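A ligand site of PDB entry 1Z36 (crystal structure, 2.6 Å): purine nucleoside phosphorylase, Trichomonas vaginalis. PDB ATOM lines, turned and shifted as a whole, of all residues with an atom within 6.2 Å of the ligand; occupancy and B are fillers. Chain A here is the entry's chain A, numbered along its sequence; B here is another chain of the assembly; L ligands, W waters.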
ATOM      1  N   GLY A  20      33.566 -22.039  11.233  1.00  0.00           N
ATOM      2  CA  GLY A  20      32.948 -22.990  12.136  1.00  0.00           C
ATOM      3  C   GLY A  20      33.928 -23.741  13.007  1.00  0.00           C
ATOM      4  O   GLY A  20      33.743 -23.844  14.220  1.00  0.00           O
ATOM      5  N   HIS A  62      32.747 -20.072  15.217  1.00  0.00           N
ATOM      6  CA  HIS A  62      31.364 -19.694  15.419  1.00  0.00           C
ATOM      7  C   HIS A  62      30.440 -20.903  15.502  1.00  0.00           C
ATOM      8  O   HIS A  62      29.224 -20.761  15.559  1.00  0.00           O
ATOM      9  CB  HIS A  62      30.870 -18.739  14.315  1.00  0.00           C
ATOM     10  CG  HIS A  62      30.948 -19.303  12.933  1.00  0.00           C
ATOM     11  ND1 HIS A  62      30.379 -20.506  12.574  1.00  0.00           N
ATOM     12  CD2 HIS A  62      31.522 -18.815  11.804  1.00  0.00           C
ATOM     13  CE1 HIS A  62      30.599 -20.738  11.296  1.00  0.00           C
ATOM     14  NE2 HIS A  62      31.289 -19.723  10.797  1.00  0.00           N
ATOM     15  N   GLY A  63      31.031 -22.105  15.531  1.00  0.00           N
ATOM     16  CA  GLY A  63      30.251 -23.327  15.615  1.00  0.00           C
ATOM     17  C   GLY A  63      29.509 -23.618  14.315  1.00  0.00           C
ATOM     18  O   GLY A  63      29.706 -22.953  13.312  1.00  0.00           O
ATOM     19  N   MET A  64      28.635 -24.621  14.335  1.00  0.00           N
ATOM     20  CA  MET A  64      27.877 -24.952  13.134  1.00  0.00           C
ATOM     21  C   MET A  64      26.404 -24.651  13.318  1.00  0.00           C
ATOM     22  O   MET A  64      25.830 -24.956  14.366  1.00  0.00           O
ATOM     23  CB  MET A  64      28.055 -26.424  12.782  1.00  0.00           C
ATOM     24  CG  MET A  64      29.497 -26.846  12.589  1.00  0.00           C
ATOM     25  SD  MET A  64      29.597 -28.579  12.097  1.00  0.00           S
ATOM     26  CE  MET A  64      28.963 -29.398  13.594  1.00  0.00           C
ATOM     27  N   GLY A  65      25.801 -24.041  12.296  1.00  0.00           N
ATOM     28  CA  GLY A  65      24.387 -23.718  12.340  1.00  0.00           C
ATOM     29  C   GLY A  65      24.051 -22.272  12.635  1.00  0.00           C
ATOM     30  O   GLY A  65      24.784 -21.576  13.328  1.00  0.00           O
ATOM     31  N   ARG A  87      32.745 -14.133   7.314  1.00  0.00           N
ATOM     32  CA  ARG A  87      32.712 -15.566   7.544  1.00  0.00           C
ATOM     33  C   ARG A  87      33.624 -16.229   6.502  1.00  0.00           C
ATOM     34  O   ARG A  87      33.552 -15.957   5.305  1.00  0.00           O
ATOM     35  CB  ARG A  87      31.286 -16.102   7.414  1.00  0.00           C
ATOM     36  CG  ARG A  87      31.143 -17.566   7.831  1.00  0.00           C
ATOM     37  CD  ARG A  87      29.794 -18.141   7.437  1.00  0.00           C
ATOM     38  NE  ARG A  87      29.944 -19.335   6.608  1.00  0.00           N
ATOM     39  CZ  ARG A  87      30.594 -20.431   6.977  1.00  0.00           C
ATOM     40  NH1 ARG A  87      31.169 -20.487   8.175  1.00  0.00           N
ATOM     41  NH2 ARG A  87      30.671 -21.480   6.159  1.00  0.00           N
ATOM     42  N   THR A  90      34.247 -23.556   4.652  1.00  0.00           N
ATOM     43  CA  THR A  90      33.963 -24.515   3.595  1.00  0.00           C
ATOM     44  C   THR A  90      32.472 -24.516   3.283  1.00  0.00           C
ATOM     45  O   THR A  90      31.681 -23.879   3.972  1.00  0.00           O
ATOM     46  CB  THR A  90      34.384 -25.924   4.010  1.00  0.00           C
ATOM     47  OG1 THR A  90      33.620 -26.335   5.143  1.00  0.00           O
ATOM     48  CG2 THR A  90      35.859 -25.958   4.387  1.00  0.00           C
ATOM     49  N   CYS A  91      32.087 -25.249   2.243  1.00  0.00           N
ATOM     50  CA  CYS A  91      30.692 -25.332   1.849  1.00  0.00           C
ATOM     51  C   CYS A  91      30.543 -26.442   0.821  1.00  0.00           C
ATOM     52  O   CYS A  91      31.551 -26.956   0.330  1.00  0.00           O
ATOM     53  CB  CYS A  91      30.229 -24.003   1.240  1.00  0.00           C
ATOM     54  SG  CYS A  91      31.167 -23.548  -0.255  1.00  0.00           S
ATOM     55  N   GLY A  92      29.309 -26.808   0.510  1.00  0.00           N
ATOM     56  CA  GLY A  92      29.074 -27.858  -0.473  1.00  0.00           C
ATOM     57  C   GLY A  92      28.508 -27.299  -1.763  1.00  0.00           C
ATOM     58  O   GLY A  92      27.501 -26.588  -1.755  1.00  0.00           O
ATOM     59  N   ALA A  93      29.154 -27.590  -2.881  1.00  0.00           N
ATOM     60  CA  ALA A  93      28.683 -27.094  -4.166  1.00  0.00           C
ATOM     61  C   ALA A  93      27.331 -27.688  -4.501  1.00  0.00           C
ATOM     62  O   ALA A  93      27.047 -28.842  -4.168  1.00  0.00           O
ATOM     63  CB  ALA A  93      29.681 -27.435  -5.276  1.00  0.00           C
ATOM     64  N   THR A 156      21.627 -24.166   5.354  1.00  0.00           N
ATOM     65  CA  THR A 156      20.681 -25.198   5.775  1.00  0.00           C
ATOM     66  C   THR A 156      20.719 -25.473   7.286  1.00  0.00           C
ATOM     67  O   THR A 156      21.725 -25.243   7.959  1.00  0.00           O
ATOM     68  CB  THR A 156      20.910 -26.532   5.021  1.00  0.00           C
ATOM     69  OG1 THR A 156      19.882 -27.475   5.373  1.00  0.00           O
ATOM     70  CG2 THR A 156      22.276 -27.143   5.368  1.00  0.00           C
ATOM     71  N   LEU A 158      19.646 -28.522   8.154  1.00  0.00           N
ATOM     72  CA  LEU A 158      19.858 -29.965   8.093  1.00  0.00           C
ATOM     73  C   LEU A 158      21.013 -30.367   7.180  1.00  0.00           C
ATOM     74  O   LEU A 158      20.831 -30.472   5.957  1.00  0.00           O
ATOM     75  CB  LEU A 158      18.593 -30.688   7.584  1.00  0.00           C
ATOM     76  CG  LEU A 158      17.363 -31.088   8.425  1.00  0.00           C
ATOM     77  CD1 LEU A 158      17.704 -31.085   9.904  1.00  0.00           C
ATOM     78  CD2 LEU A 158      16.203 -30.164   8.110  1.00  0.00           C
ATOM     79  N   PHE A 159      22.185 -30.615   7.751  1.00  0.00           N
ATOM     80  CA  PHE A 159      23.330 -31.056   6.946  1.00  0.00           C
ATOM     81  C   PHE A 159      22.837 -32.312   6.202  1.00  0.00           C
ATOM     82  O   PHE A 159      23.051 -32.444   4.995  1.00  0.00           O
ATOM     83  CB  PHE A 159      24.504 -31.405   7.857  1.00  0.00           C
ATOM     84  CG  PHE A 159      25.710 -31.921   7.119  1.00  0.00           C
ATOM     85  CD1 PHE A 159      26.698 -31.040   6.670  1.00  0.00           C
ATOM     86  CD2 PHE A 159      25.862 -33.289   6.891  1.00  0.00           C
ATOM     87  CE1 PHE A 159      27.842 -31.522   6.024  1.00  0.00           C
ATOM     88  CE2 PHE A 159      26.995 -33.778   6.251  1.00  0.00           C
ATOM     89  CZ  PHE A 159      27.998 -32.890   5.805  1.00  0.00           C
ATOM     90  N   VAL A 178      26.174 -24.630  -0.378  1.00  0.00           N
ATOM     91  CA  VAL A 178      25.467 -24.716   0.878  1.00  0.00           C
ATOM     92  C   VAL A 178      26.411 -24.746   2.067  1.00  0.00           C
ATOM     93  O   VAL A 178      27.429 -25.432   2.040  1.00  0.00           O
ATOM     94  CB  VAL A 178      24.572 -25.970   0.929  1.00  0.00           C
ATOM     95  CG1 VAL A 178      24.222 -26.333   2.375  1.00  0.00           C
ATOM     96  CG2 VAL A 178      23.299 -25.718   0.150  1.00  0.00           C
ATOM     97  N   GLU A 179      26.057 -23.979   3.084  1.00  0.00           N
ATOM     98  CA  GLU A 179      26.810 -23.941   4.334  1.00  0.00           C
ATOM     99  C   GLU A 179      25.750 -23.817   5.437  1.00  0.00           C
ATOM    100  O   GLU A 179      24.589 -24.165   5.201  1.00  0.00           O
ATOM    101  CB  GLU A 179      27.828 -22.778   4.344  1.00  0.00           C
ATOM    102  CG  GLU A 179      27.364 -21.441   3.779  1.00  0.00           C
ATOM    103  CD  GLU A 179      26.348 -20.752   4.668  1.00  0.00           C
ATOM    104  OE1 GLU A 179      25.141 -21.004   4.489  1.00  0.00           O
ATOM    105  OE2 GLU A 179      26.766 -19.972   5.567  1.00  0.00           O
ATOM    106  N   MET A 180      26.108 -23.332   6.623  1.00  0.00           N
ATOM    107  CA  MET A 180      25.103 -23.302   7.686  1.00  0.00           C
ATOM    108  C   MET A 180      25.076 -22.071   8.587  1.00  0.00           C
ATOM    109  O   MET A 180      24.649 -22.161   9.734  1.00  0.00           O
ATOM    110  CB  MET A 180      25.271 -24.561   8.559  1.00  0.00           C
ATOM    111  CG  MET A 180      25.158 -25.870   7.786  1.00  0.00           C
ATOM    112  SD  MET A 180      25.374 -27.403   8.761  1.00  0.00           S
ATOM    113  CE  MET A 180      23.956 -27.362   9.861  1.00  0.00           C
ATOM    114  N   GLU A 181      25.520 -20.922   8.102  1.00  0.00           N
ATOM    115  CA  GLU A 181      25.556 -19.765   8.969  1.00  0.00           C
ATOM    116  C   GLU A 181      25.185 -18.418   8.348  1.00  0.00           C
ATOM    117  O   GLU A 181      24.486 -17.617   8.969  1.00  0.00           O
ATOM    118  CB  GLU A 181      26.951 -19.655   9.604  1.00  0.00           C
ATOM    119  CG  GLU A 181      27.361 -20.849  10.458  1.00  0.00           C
ATOM    120  CD  GLU A 181      27.746 -22.075   9.644  1.00  0.00           C
ATOM    121  OE1 GLU A 181      27.764 -23.189  10.221  1.00  0.00           O
ATOM    122  OE2 GLU A 181      28.049 -21.935   8.439  1.00  0.00           O
ATOM    123  N   SER A 203      34.304 -27.813  -0.392  1.00  0.00           N
ATOM    124  CA  SER A 203      34.976 -29.006   0.097  1.00  0.00           C
ATOM    125  C   SER A 203      34.351 -30.269  -0.475  1.00  0.00           C
ATOM    126  O   SER A 203      34.983 -31.326  -0.511  1.00  0.00           O
ATOM    127  CB  SER A 203      34.912 -29.054   1.625  1.00  0.00           C
ATOM    128  OG  SER A 203      33.564 -29.066   2.066  1.00  0.00           O
ATOM    129  N   ASP A 204      33.104 -30.159  -0.933  1.00  0.00           N
ATOM    130  CA  ASP A 204      32.397 -31.297  -1.499  1.00  0.00           C
ATOM    131  C   ASP A 204      31.269 -30.848  -2.430  1.00  0.00           C
ATOM    132  O   ASP A 204      30.862 -29.688  -2.397  1.00  0.00           O
ATOM    133  CB  ASP A 204      31.806 -32.170  -0.383  1.00  0.00           C
ATOM    134  CG  ASP A 204      30.737 -31.451   0.439  1.00  0.00           C
ATOM    135  OD1 ASP A 204      31.087 -30.565   1.261  1.00  0.00           O
ATOM    136  OD2 ASP A 204      29.538 -31.769   0.251  1.00  0.00           O
ATOM    137  N   ILE A 206      27.368 -31.752  -3.520  1.00  0.00           N
ATOM    138  CA  ILE A 206      26.220 -32.536  -3.093  1.00  0.00           C
ATOM    139  C   ILE A 206      25.466 -33.240  -4.218  1.00  0.00           C
ATOM    140  O   ILE A 206      24.686 -34.166  -3.961  1.00  0.00           O
ATOM    141  CB  ILE A 206      25.208 -31.683  -2.264  1.00  0.00           C
ATOM    142  CG1 ILE A 206      24.384 -30.801  -3.186  1.00  0.00           C
ATOM    143  CG2 ILE A 206      25.950 -30.840  -1.245  1.00  0.00           C
ATOM    144  CD1 ILE A 206      23.341 -29.972  -2.462  1.00  0.00           C
ATOM    145  N   PRO B   3      32.340 -36.582   8.255  1.00  0.00           N
ATOM    146  CA  PRO B   3      32.925 -35.247   8.086  1.00  0.00           C
ATOM    147  C   PRO B   3      33.152 -34.546   9.413  1.00  0.00           C
ATOM    148  O   PRO B   3      33.855 -33.531   9.462  1.00  0.00           O
ATOM    149  CB  PRO B   3      31.874 -34.515   7.251  1.00  0.00           C
ATOM    150  CG  PRO B   3      31.227 -35.627   6.465  1.00  0.00           C
ATOM    151  CD  PRO B   3      31.078 -36.707   7.493  1.00  0.00           C
ATOM    152  N   HIS B   4      32.577 -35.075  10.492  1.00  0.00           N
ATOM    153  CA  HIS B   4      32.706 -34.448  11.805  1.00  0.00           C
ATOM    154  C   HIS B   4      33.270 -35.385  12.875  1.00  0.00           C
ATOM    155  O   HIS B   4      33.393 -35.004  14.045  1.00  0.00           O
ATOM    156  CB  HIS B   4      31.340 -33.917  12.273  1.00  0.00           C
ATOM    157  CG  HIS B   4      30.598 -33.156  11.213  1.00  0.00           C
ATOM    158  ND1 HIS B   4      29.773 -33.769  10.301  1.00  0.00           N
ATOM    159  CD2 HIS B   4      30.624 -31.847  10.876  1.00  0.00           C
ATOM    160  CE1 HIS B   4      29.334 -32.873   9.442  1.00  0.00           C
ATOM    161  NE2 HIS B   4      29.834 -31.702   9.770  1.00  0.00           N
ATOM    162  N   ARG B  43      37.207 -30.609  14.958  1.00  0.00           N
ATOM    163  CA  ARG B  43      36.564 -29.349  15.369  1.00  0.00           C
ATOM    164  C   ARG B  43      36.616 -29.157  16.878  1.00  0.00           C
ATOM    165  O   ARG B  43      35.725 -28.529  17.448  1.00  0.00           O
ATOM    166  CB  ARG B  43      35.110 -29.307  14.903  1.00  0.00           C
ATOM    167  CG  ARG B  43      34.953 -29.251  13.411  1.00  0.00           C
ATOM    168  CD  ARG B  43      33.527 -29.586  12.976  1.00  0.00           C
ATOM    169  NE  ARG B  43      33.344 -29.322  11.555  1.00  0.00           N
ATOM    170  CZ  ARG B  43      33.127 -28.114  11.052  1.00  0.00           C
ATOM    171  NH1 ARG B  43      33.057 -27.059  11.856  1.00  0.00           N
ATOM    172  NH2 ARG B  43      32.993 -27.945   9.738  1.00  0.00           N
ATOM    173  N   ILE B  71      23.601 -32.890  13.600  1.00  0.00           N
ATOM    174  CA  ILE B  71      24.687 -33.478  12.824  1.00  0.00           C
ATOM    175  C   ILE B  71      25.318 -34.625  13.604  1.00  0.00           C
ATOM    176  O   ILE B  71      25.411 -35.758  13.118  1.00  0.00           O
ATOM    177  CB  ILE B  71      25.773 -32.447  12.515  1.00  0.00           C
ATOM    178  CG1 ILE B  71      25.297 -31.466  11.455  1.00  0.00           C
ATOM    179  CG2 ILE B  71      27.052 -33.172  12.071  1.00  0.00           C
ATOM    180  CD1 ILE B  71      26.265 -30.334  11.192  1.00  0.00           C
HETATM  181  N1  LIG L   1      26.563 -28.753   3.632  1.00  0.00           N
HETATM  182  C1  LIG L   1      26.337 -27.998   4.689  1.00  0.00           C
HETATM  183  N2  LIG L   1      27.315 -27.372   5.318  1.00  0.00           N
HETATM  184  C2  LIG L   1      28.584 -27.507   4.883  1.00  0.00           C
HETATM  185  C3  LIG L   1      28.861 -28.293   3.782  1.00  0.00           C
HETATM  186  C4  LIG L   1      27.797 -28.931   3.150  1.00  0.00           C
HETATM  187  N3  LIG L   1      28.006 -29.685   2.078  1.00  0.00           N
HETATM  188  N4  LIG L   1      30.180 -28.256   3.595  1.00  0.00           N
HETATM  189  N5  LIG L   1      30.732 -27.549   4.438  1.00  0.00           N
HETATM  190  C5  LIG L   1      29.827 -27.053   5.281  1.00  0.00           C
HETATM  191  C6  LIG L   1      30.156 -26.159   6.489  1.00  0.00           C
HETATM  192  C7  LIG L   1      28.907 -25.565   7.151  1.00  0.00           C
HETATM  193  O1  LIG L   1      28.941 -24.132   7.132  1.00  0.00           O
HETATM  194  C8  LIG L   1      28.945 -26.085   8.585  1.00  0.00           C
HETATM  195  O2  LIG L   1      29.546 -25.115   9.448  1.00  0.00           O
HETATM  196  C9  LIG L   1      29.821 -27.332   8.463  1.00  0.00           C
HETATM  197  O3  LIG L   1      30.820 -26.930   7.508  1.00  0.00           O
HETATM  198  C10 LIG L   1      29.044 -28.570   7.993  1.00  0.00           C
HETATM  199  O4  LIG L   1      29.956 -29.650   7.806  1.00  0.00           O
HETATM  200  O   HOH W   1      23.533 -30.296   3.210  1.00  0.00           O
HETATM  201  O   HOH W   2      32.633 -29.997   6.556  1.00  0.00           O
HETATM  202  O   HOH W   3      32.022 -24.963   9.841  1.00  0.00           O
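Water W3 lies within hydrogen-bond range of an oxygen (O2) of the ligand and the guanidinium group of Arg 43 of chain B. Water W1 bridges the backbone carbonyl oxygen (O) of Phe 159 and a nitrogen (N1) of the ligand.
O of Gly 92 sits at hydrogen-bond distance from N of Val 178, at 2.7 Å. The side-chain carboxylate (OE2) of Glu 181 lies within salt-bridge range of the guanidinium group (NH1) of Arg 87. OG of Ser 203 lies within hydrogen-bond range of OD1 of Asp 204 (3.0 Å). A ring nitrogen (NE2) of His 62 is in hydrogen-bond range of the guanidinium group of Arg 87 (2.7 Å). The side-chain carboxylate of Glu 179 lies within salt-bridge range of the guanidinium group of Arg 87 (3.4 Å). O of Met 180 lies close to N of Gly 65 (3.4 Å). N of Thr 156 sits at hydrogen-bond distance from O of Glu 179 (3.0 Å). OE1 of Glu 181 is in hydrogen-bond range of N of Gly 65 (3.0 Å).
An oxygen (O3) of the ligand is in hydrogen-bond range of the guanidinium group (NH2) of Arg 43 of chain B, 3.3 Å away. O4 of the ligand lies within hydrogen-bond range of NE2 of His 4 of chain B (2.8 Å). OE2 of Glu 181 lies within hydrogen-bond range of O1 of the ligand (2.7 Å). The side-chain carboxylate (OD2) of Asp 204 is in hydrogen-bond range of a nitrogen (N3) of the ligand (3.2 Å). NH2 of Arg 87 is in hydrogen-bond range of O1 of the ligand (3.3 Å). N5 of the ligand is in hydrogen-bond range of OG1 of Thr 90 (3.2 Å). The backbone NH of Met 180 is in hydrogen-bond range of an oxygen (O1) of the ligand (3.0 Å). N of Cys 91 sits close to N5 of the ligand (3.5 Å).
Merely in contact with the ligand: Glu 179 (3.3 Å), Gly 92 (3.3 Å), Phe 159 (3.3 Å), Val 178 (3.5 Å), Met 64 (3.6 Å) and Ser 203 (3.8 Å). Hydrophobic or aromatic side chains that line the ligand: Met 64, Phe 159, Val 178, Met 180 and His 4 of chain B.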
